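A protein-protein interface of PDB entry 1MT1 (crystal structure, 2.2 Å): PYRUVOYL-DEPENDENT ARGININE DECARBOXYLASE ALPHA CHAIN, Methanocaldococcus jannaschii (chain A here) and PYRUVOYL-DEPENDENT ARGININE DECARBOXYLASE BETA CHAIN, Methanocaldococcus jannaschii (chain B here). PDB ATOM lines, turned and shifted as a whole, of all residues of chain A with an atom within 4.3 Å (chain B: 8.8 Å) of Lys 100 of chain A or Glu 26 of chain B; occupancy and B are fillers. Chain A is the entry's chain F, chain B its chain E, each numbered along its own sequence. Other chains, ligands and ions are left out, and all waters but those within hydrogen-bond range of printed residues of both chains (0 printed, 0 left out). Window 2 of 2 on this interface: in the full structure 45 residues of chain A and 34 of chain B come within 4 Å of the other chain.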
ATOM      1  N   SER A  30      10.562 -20.980 -11.480  1.00  0.00           N
ATOM      2  CA  SER A  30      10.587 -19.526 -11.457  1.00  0.00           C
ATOM      3  C   SER A  30      11.976 -18.980 -11.758  1.00  0.00           C
ATOM      4  O   SER A  30      12.985 -19.554 -11.340  1.00  0.00           O
ATOM      5  CB  SER A  30      10.119 -19.005 -10.096  1.00  0.00           C
ATOM      6  OG  SER A  30      10.344 -17.609  -9.987  1.00  0.00           O
ATOM      7  N   ASP A  31      12.015 -17.868 -12.483  1.00  0.00           N
ATOM      8  CA  ASP A  31      13.275 -17.212 -12.824  1.00  0.00           C
ATOM      9  C   ASP A  31      13.399 -15.849 -12.133  1.00  0.00           C
ATOM     10  O   ASP A  31      14.216 -15.013 -12.535  1.00  0.00           O
ATOM     11  CB  ASP A  31      13.429 -17.070 -14.345  1.00  0.00           C
ATOM     12  CG  ASP A  31      12.233 -16.390 -15.011  1.00  0.00           C
ATOM     13  OD1 ASP A  31      11.273 -15.993 -14.312  1.00  0.00           O
ATOM     14  OD2 ASP A  31      12.251 -16.257 -16.252  1.00  0.00           O
ATOM     15  N   HIS A  96      11.921 -23.634  -2.236  1.00  0.00           N
ATOM     16  CA  HIS A  96      13.160 -23.218  -2.877  1.00  0.00           C
ATOM     17  C   HIS A  96      13.203 -21.710  -3.074  1.00  0.00           C
ATOM     18  O   HIS A  96      12.253 -21.115  -3.568  1.00  0.00           O
ATOM     19  CB  HIS A  96      13.288 -23.917  -4.243  1.00  0.00           C
ATOM     20  CG  HIS A  96      14.562 -23.613  -4.971  1.00  0.00           C
ATOM     21  ND1 HIS A  96      15.728 -24.321  -4.763  1.00  0.00           N
ATOM     22  CD2 HIS A  96      14.850 -22.690  -5.919  1.00  0.00           C
ATOM     23  CE1 HIS A  96      16.677 -23.846  -5.550  1.00  0.00           C
ATOM     24  NE2 HIS A  96      16.170 -22.856  -6.260  1.00  0.00           N
ATOM     25  N   VAL A  98      14.621 -19.002  -5.179  1.00  0.00           N
ATOM     26  CA  VAL A  98      15.260 -18.834  -6.474  1.00  0.00           C
ATOM     27  C   VAL A  98      16.481 -17.922  -6.423  1.00  0.00           C
ATOM     28  O   VAL A  98      16.479 -16.910  -5.723  1.00  0.00           O
ATOM     29  CB  VAL A  98      14.279 -18.257  -7.515  1.00  0.00           C
ATOM     30  CG1 VAL A  98      14.957 -18.167  -8.879  1.00  0.00           C
ATOM     31  CG2 VAL A  98      13.030 -19.113  -7.601  1.00  0.00           C
ATOM     32  N   GLU A  99      17.539 -18.326  -7.120  1.00  0.00           N
ATOM     33  CA  GLU A  99      18.756 -17.526  -7.214  1.00  0.00           C
ATOM     34  C   GLU A  99      18.695 -16.870  -8.591  1.00  0.00           C
ATOM     35  O   GLU A  99      18.722 -15.651  -8.710  1.00  0.00           O
ATOM     36  CB  GLU A  99      20.002 -18.403  -7.082  1.00  0.00           C
ATOM     37  CG  GLU A  99      20.216 -18.953  -5.682  1.00  0.00           C
ATOM     38  CD  GLU A  99      21.296 -20.026  -5.620  1.00  0.00           C
ATOM     39  OE1 GLU A  99      22.456 -19.750  -6.014  1.00  0.00           O
ATOM     40  OE2 GLU A  99      20.979 -21.153  -5.175  1.00  0.00           O
ATOM     41  N   LYS A 100      18.538 -17.697  -9.621  1.00  0.00           N
ATOM     42  CA  LYS A 100      18.434 -17.225 -10.997  1.00  0.00           C
ATOM     43  C   LYS A 100      17.267 -17.936 -11.685  1.00  0.00           C
ATOM     44  O   LYS A 100      16.407 -17.290 -12.283  1.00  0.00           O
ATOM     45  CB  LYS A 100      19.738 -17.488 -11.761  1.00  0.00           C
ATOM     46  CG  LYS A 100      20.974 -16.841 -11.128  1.00  0.00           C
ATOM     47  CD  LYS A 100      22.207 -16.959 -12.023  1.00  0.00           C
ATOM     48  CE  LYS A 100      22.157 -15.990 -13.200  1.00  0.00           C
ATOM     49  NZ  LYS A 100      22.118 -14.552 -12.780  1.00  0.00           N
ATOM     50  N   LEU A 101      17.239 -19.265 -11.569  1.00  0.00           N
ATOM     51  CA  LEU A 101      16.195 -20.103 -12.161  1.00  0.00           C
ATOM     52  C   LEU A 101      16.106 -21.381 -11.316  1.00  0.00           C
ATOM     53  O   LEU A 101      17.026 -22.198 -11.320  1.00  0.00           O
ATOM     54  CB  LEU A 101      16.568 -20.456 -13.609  1.00  0.00           C
ATOM     55  CG  LEU A 101      15.465 -20.679 -14.645  1.00  0.00           C
ATOM     56  CD1 LEU A 101      16.095 -21.118 -15.962  1.00  0.00           C
ATOM     57  CD2 LEU A 101      14.483 -21.727 -14.174  1.00  0.00           C
ATOM     58  N   GLY A 102      15.010 -21.542 -10.581  1.00  0.00           N
ATOM     59  CA  GLY A 102      14.864 -22.710  -9.732  1.00  0.00           C
ATOM     60  C   GLY A 102      13.565 -23.471  -9.907  1.00  0.00           C
ATOM     61  O   GLY A 102      12.591 -22.947 -10.434  1.00  0.00           O
ATOM     62  N   GLY B  23      12.006 -32.424  -3.911  1.00  0.00           N
ATOM     63  CA  GLY B  23      13.329 -31.886  -4.156  1.00  0.00           C
ATOM     64  C   GLY B  23      13.259 -30.540  -4.831  1.00  0.00           C
ATOM     65  O   GLY B  23      12.203 -30.141  -5.320  1.00  0.00           O
ATOM     66  N   SER B  24      14.389 -29.845  -4.871  1.00  0.00           N
ATOM     67  CA  SER B  24      14.453 -28.537  -5.493  1.00  0.00           C
ATOM     68  C   SER B  24      15.819 -28.363  -6.126  1.00  0.00           C
ATOM     69  O   SER B  24      16.784 -29.034  -5.745  1.00  0.00           O
ATOM     70  CB  SER B  24      14.223 -27.438  -4.452  1.00  0.00           C
ATOM     71  OG  SER B  24      15.258 -27.439  -3.477  1.00  0.00           O
ATOM     72  N   SER B  25      15.912 -27.457  -7.089  1.00  0.00           N
ATOM     73  CA  SER B  25      17.188 -27.238  -7.735  1.00  0.00           C
ATOM     74  C   SER B  25      17.235 -26.060  -8.676  1.00  0.00           C
ATOM     75  O   SER B  25      16.223 -25.647  -9.255  1.00  0.00           O
ATOM     76  CB  SER B  25      17.608 -28.495  -8.510  1.00  0.00           C
ATOM     77  OG  SER B  25      18.811 -28.305  -9.239  1.00  0.00           O
ATOM     78  N   GLU B  26      18.439 -25.522  -8.805  1.00  0.00           N
ATOM     79  CA  GLU B  26      18.738 -24.399  -9.676  1.00  0.00           C
ATOM     80  C   GLU B  26      19.113 -25.050 -11.019  1.00  0.00           C
ATOM     81  O   GLU B  26      19.454 -26.236 -11.052  1.00  0.00           O
ATOM     82  CB  GLU B  26      19.925 -23.642  -9.069  1.00  0.00           C
ATOM     83  CG  GLU B  26      20.035 -22.169  -9.406  1.00  0.00           C
ATOM     84  CD  GLU B  26      18.852 -21.324  -8.952  1.00  0.00           C
ATOM     85  OE1 GLU B  26      18.204 -21.602  -7.921  1.00  0.00           O
ATOM     86  OE2 GLU B  26      18.582 -20.341  -9.649  1.00  0.00           O
ATOM     87  N   GLY B  27      19.024 -24.303 -12.121  1.00  0.00           N
ATOM     88  CA  GLY B  27      19.358 -24.863 -13.425  1.00  0.00           C
ATOM     89  C   GLY B  27      19.522 -23.801 -14.493  1.00  0.00           C
ATOM     90  O   GLY B  27      18.975 -22.705 -14.363  1.00  0.00           O
ATOM     91  N   GLU B  28      20.256 -24.126 -15.556  1.00  0.00           N
ATOM     92  CA  GLU B  28      20.486 -23.181 -16.648  1.00  0.00           C
ATOM     93  C   GLU B  28      19.263 -22.977 -17.538  1.00  0.00           C
ATOM     94  O   GLU B  28      19.131 -21.950 -18.193  1.00  0.00           O
ATOM     95  CB  GLU B  28      21.728 -23.582 -17.459  1.00  0.00           C
ATOM     96  CG  GLU B  28      23.024 -23.463 -16.645  1.00  0.00           C
ATOM     97  CD  GLU B  28      24.283 -23.800 -17.433  1.00  0.00           C
ATOM     98  OE1 GLU B  28      24.905 -24.846 -17.135  1.00  0.00           O
ATOM     99  OE2 GLU B  28      24.671 -23.009 -18.327  1.00  0.00           O
ATOM    100  N   THR B  29      18.380 -23.969 -17.577  1.00  0.00           N
ATOM    101  CA  THR B  29      17.143 -23.882 -18.351  1.00  0.00           C
ATOM    102  C   THR B  29      16.055 -24.461 -17.465  1.00  0.00           C
ATOM    103  O   THR B  29      16.351 -25.111 -16.460  1.00  0.00           O
ATOM    104  CB  THR B  29      17.167 -24.726 -19.651  1.00  0.00           C
ATOM    105  OG1 THR B  29      17.262 -26.115 -19.321  1.00  0.00           O
ATOM    106  CG2 THR B  29      18.318 -24.324 -20.559  1.00  0.00           C
ATOM    107  N   PRO B  30      14.782 -24.218 -17.809  1.00  0.00           N
ATOM    108  CA  PRO B  30      13.672 -24.745 -17.011  1.00  0.00           C
ATOM    109  C   PRO B  30      13.727 -26.273 -16.894  1.00  0.00           C
ATOM    110  O   PRO B  30      13.536 -26.823 -15.811  1.00  0.00           O
ATOM    111  CB  PRO B  30      12.445 -24.280 -17.798  1.00  0.00           C
ATOM    112  CG  PRO B  30      12.896 -22.965 -18.363  1.00  0.00           C
ATOM    113  CD  PRO B  30      14.292 -23.301 -18.856  1.00  0.00           C
ATOM    114  N   LEU B  31      14.038 -26.948 -17.999  1.00  0.00           N
ATOM    115  CA  LEU B  31      14.122 -28.406 -18.018  1.00  0.00           C
ATOM    116  C   LEU B  31      15.306 -28.904 -17.195  1.00  0.00           C
ATOM    117  O   LEU B  31      15.196 -29.901 -16.476  1.00  0.00           O
ATOM    118  CB  LEU B  31      14.238 -28.925 -19.454  1.00  0.00           C
ATOM    119  CG  LEU B  31      14.013 -30.435 -19.589  1.00  0.00           C
ATOM    120  CD1 LEU B  31      12.591 -30.754 -19.139  1.00  0.00           C
ATOM    121  CD2 LEU B  31      14.233 -30.897 -21.022  1.00  0.00           C
ATOM    122  N   ASN B  32      16.439 -28.214 -17.296  1.00  0.00           N
ATOM    123  CA  ASN B  32      17.612 -28.608 -16.524  1.00  0.00           C
ATOM    124  C   ASN B  32      17.355 -28.431 -15.029  1.00  0.00           C
ATOM    125  O   ASN B  32      17.830 -29.235 -14.216  1.00  0.00           O
ATOM    126  CB  ASN B  32      18.847 -27.825 -16.963  1.00  0.00           C
ATOM    127  CG  ASN B  32      19.412 -28.326 -18.286  1.00  0.00           C
ATOM    128  OD1 ASN B  32      19.849 -29.471 -18.392  1.00  0.00           O
ATOM    129  ND2 ASN B  32      19.407 -27.471 -19.293  1.00  0.00           N
ATOM    130  N   ALA B  33      16.590 -27.398 -14.667  1.00  0.00           N
ATOM    131  CA  ALA B  33      16.253 -27.142 -13.261  1.00  0.00           C
ATOM    132  C   ALA B  33      15.319 -28.255 -12.805  1.00  0.00           C
ATOM    133  O   ALA B  33      15.496 -28.826 -11.737  1.00  0.00           O
ATOM    134  CB  ALA B  33      15.574 -25.775 -13.106  1.00  0.00           C
ATOM    135  N   PHE B  34      14.338 -28.581 -13.643  1.00  0.00           N
ATOM    136  CA  PHE B  34      13.402 -29.653 -13.341  1.00  0.00           C
ATOM    137  C   PHE B  34      14.206 -30.953 -13.156  1.00  0.00           C
ATOM    138  O   PHE B  34      14.051 -31.646 -12.153  1.00  0.00           O
ATOM    139  CB  PHE B  34      12.395 -29.789 -14.486  1.00  0.00           C
ATOM    140  CG  PHE B  34      11.403 -30.901 -14.300  1.00  0.00           C
ATOM    141  CD1 PHE B  34      10.333 -30.755 -13.430  1.00  0.00           C
ATOM    142  CD2 PHE B  34      11.526 -32.090 -15.018  1.00  0.00           C
ATOM    143  CE1 PHE B  34       9.394 -31.778 -13.276  1.00  0.00           C
ATOM    144  CE2 PHE B  34      10.596 -33.114 -14.869  1.00  0.00           C
ATOM    145  CZ  PHE B  34       9.528 -32.958 -13.997  1.00  0.00           C
ATOM    146  N   ASP B  35      15.111 -31.232 -14.095  1.00  0.00           N
ATOM    147  CA  ASP B  35      15.958 -32.428 -14.048  1.00  0.00           C
ATOM    148  C   ASP B  35      16.738 -32.490 -12.724  1.00  0.00           C
ATOM    149  O   ASP B  35      16.779 -33.536 -12.065  1.00  0.00           O
ATOM    150  CB  ASP B  35      16.918 -32.434 -15.250  1.00  0.00           C
ATOM    151  CG  ASP B  35      17.724 -33.728 -15.368  1.00  0.00           C
ATOM    152  OD1 ASP B  35      17.131 -34.829 -15.298  1.00  0.00           O
ATOM    153  OD2 ASP B  35      18.959 -33.641 -15.557  1.00  0.00           O
ATOM    154  N   GLY B  36      17.317 -31.359 -12.322  1.00  0.00           N
ATOM    155  CA  GLY B  36      18.062 -31.306 -11.074  1.00  0.00           C
ATOM    156  C   GLY B  36      17.195 -31.533  -9.841  1.00  0.00           C
ATOM    157  O   GLY B  36      17.666 -32.071  -8.842  1.00  0.00           O
ATOM    158  N   ALA B  37      15.941 -31.085  -9.887  1.00  0.00           N
ATOM    159  CA  ALA B  37      15.031 -31.271  -8.763  1.00  0.00           C
ATOM    160  C   ALA B  37      14.671 -32.755  -8.615  1.00  0.00           C
ATOM    161  O   ALA B  37      14.500 -33.241  -7.499  1.00  0.00           O
ATOM    162  CB  ALA B  37      13.777 -30.434  -8.949  1.00  0.00           C
ATOM    163  N   LEU B  39      16.647 -35.290  -9.447  1.00  0.00           N
ATOM    164  CA  LEU B  39      17.849 -35.923  -8.900  1.00  0.00           C
ATOM    165  C   LEU B  39      17.947 -35.649  -7.403  1.00  0.00           C
ATOM    166  O   LEU B  39      18.256 -36.546  -6.617  1.00  0.00           O
ATOM    167  CB  LEU B  39      19.103 -35.391  -9.599  1.00  0.00           C
ATOM    168  CG  LEU B  39      19.295 -35.809 -11.056  1.00  0.00           C
ATOM    169  CD1 LEU B  39      20.241 -34.842 -11.773  1.00  0.00           C
ATOM    170  CD2 LEU B  39      19.805 -37.244 -11.115  1.00  0.00           C
ATOM    171  N   ASN B  40      17.691 -34.402  -7.021  1.00  0.00           N
ATOM    172  CA  ASN B  40      17.725 -33.991  -5.619  1.00  0.00           C
ATOM    173  C   ASN B  40      16.668 -34.792  -4.852  1.00  0.00           C
ATOM    174  O   ASN B  40      16.827 -35.077  -3.669  1.00  0.00           O
ATOM    175  CB  ASN B  40      17.447 -32.486  -5.515  1.00  0.00           C
ATOM    176  CG  ASN B  40      17.565 -31.961  -4.093  1.00  0.00           C
ATOM    177  OD1 ASN B  40      16.564 -31.598  -3.463  1.00  0.00           O
ATOM    178  ND2 ASN B  40      18.790 -31.903  -3.581  1.00  0.00           N
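ND1 of His 96 of chain A is in hydrogen-bond range of OG of Ser 24 of chain B (3.4 Å).
OE1 of Glu 26 of chain B sits at hydrogen-bond distance from NE2 of His 96 of chain A, 2.9 Å away.
OE2 of Glu 26 of chain B lies within hydrogen-bond range of N of Glu 99 of chain A (3.4 Å).
N of Lys 100 of chain A sits at hydrogen-bond distance from OE2 of Glu 26 of chain B (2.6 Å).
N of Leu 101 of chain A sits at hydrogen-bond distance from OE2 of Glu 26 of chain B (2.6 Å).
The backbone NH of Gly 27 of chain B sits at hydrogen-bond distance from the backbone carbonyl oxygen of Leu 101 of chain A, 3.0 Å away.
The side-chain amide oxygen (OD1) of Asn 40 of chain B sits at hydrogen-bond distance from the backbone NH (N) of Ser 24 of chain B (3.1 Å).
The side-chain amide nitrogen (ND2) of Asn 32 of chain B lies within hydrogen-bond range of the side-chain hydroxyl (OG1) of Thr 29 of chain B (2.5 Å).
The backbone NH of Gly 102 of chain A lies within hydrogen-bond range of the backbone carbonyl oxygen of Ser 30 of chain A (2.9 Å).
Among the printed residues, pairs that only touch across the chains: His 96 of chain A with Ser 25 of chain B, Leu 101 of chain A with Glu 28 of chain B, Leu 101 of chain A with Thr 29 of chain B, Leu 101 of chain A with Pro 30 of chain B, Gly 102 of chain A with Ser 25 of chain B and Gly 102 of chain A with Glu 26 of chain B.
Of the printed residues of chain A, Glu 26 of chain B touches His 96, Glu 99, Lys 100, Leu 101 and Gly 102.
Of the printed residues of chain B, Gly 102 of chain A touches Ser 25 (3.3 Å) and Glu 26 (3.9 Å).
Of the printed residues of chain B, Leu 101 of chain A touches Glu 26 (2.6 Å), Gly 27 (3.0 Å), Glu 28 (3.9 Å), Thr 29 (3.7 Å) and Pro 30 (3.8 Å).
Of the printed residues of chain B, His 96 of chain A touches Ser 24, Ser 25 and Glu 26.
Of the printed residues of chain A, Pro 30 of chain B touches Leu 101.
Ala 33 of chain B touches none of the printed residues of chain A.
Leu 31 of chain B touches none of the printed residues of chain A.
The nearest printed residue of chain B that does not touch Lys 100 of chain A is Gly 27 of chain B (5.7 Å).
The nearest printed residue of chain A that does not touch Glu 26 of chain B is Val 98 of chain A (4.3 Å).
Of the 17 printed residues of chain B, 7 touch a printed residue of chain A.
Along chain B the printed residues that touch a printed residue of chain A span positions 24 to 30.
Hydrophobic or aromatic side chains of chain A that line the printed part of chain B: His 96 and Leu 101.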
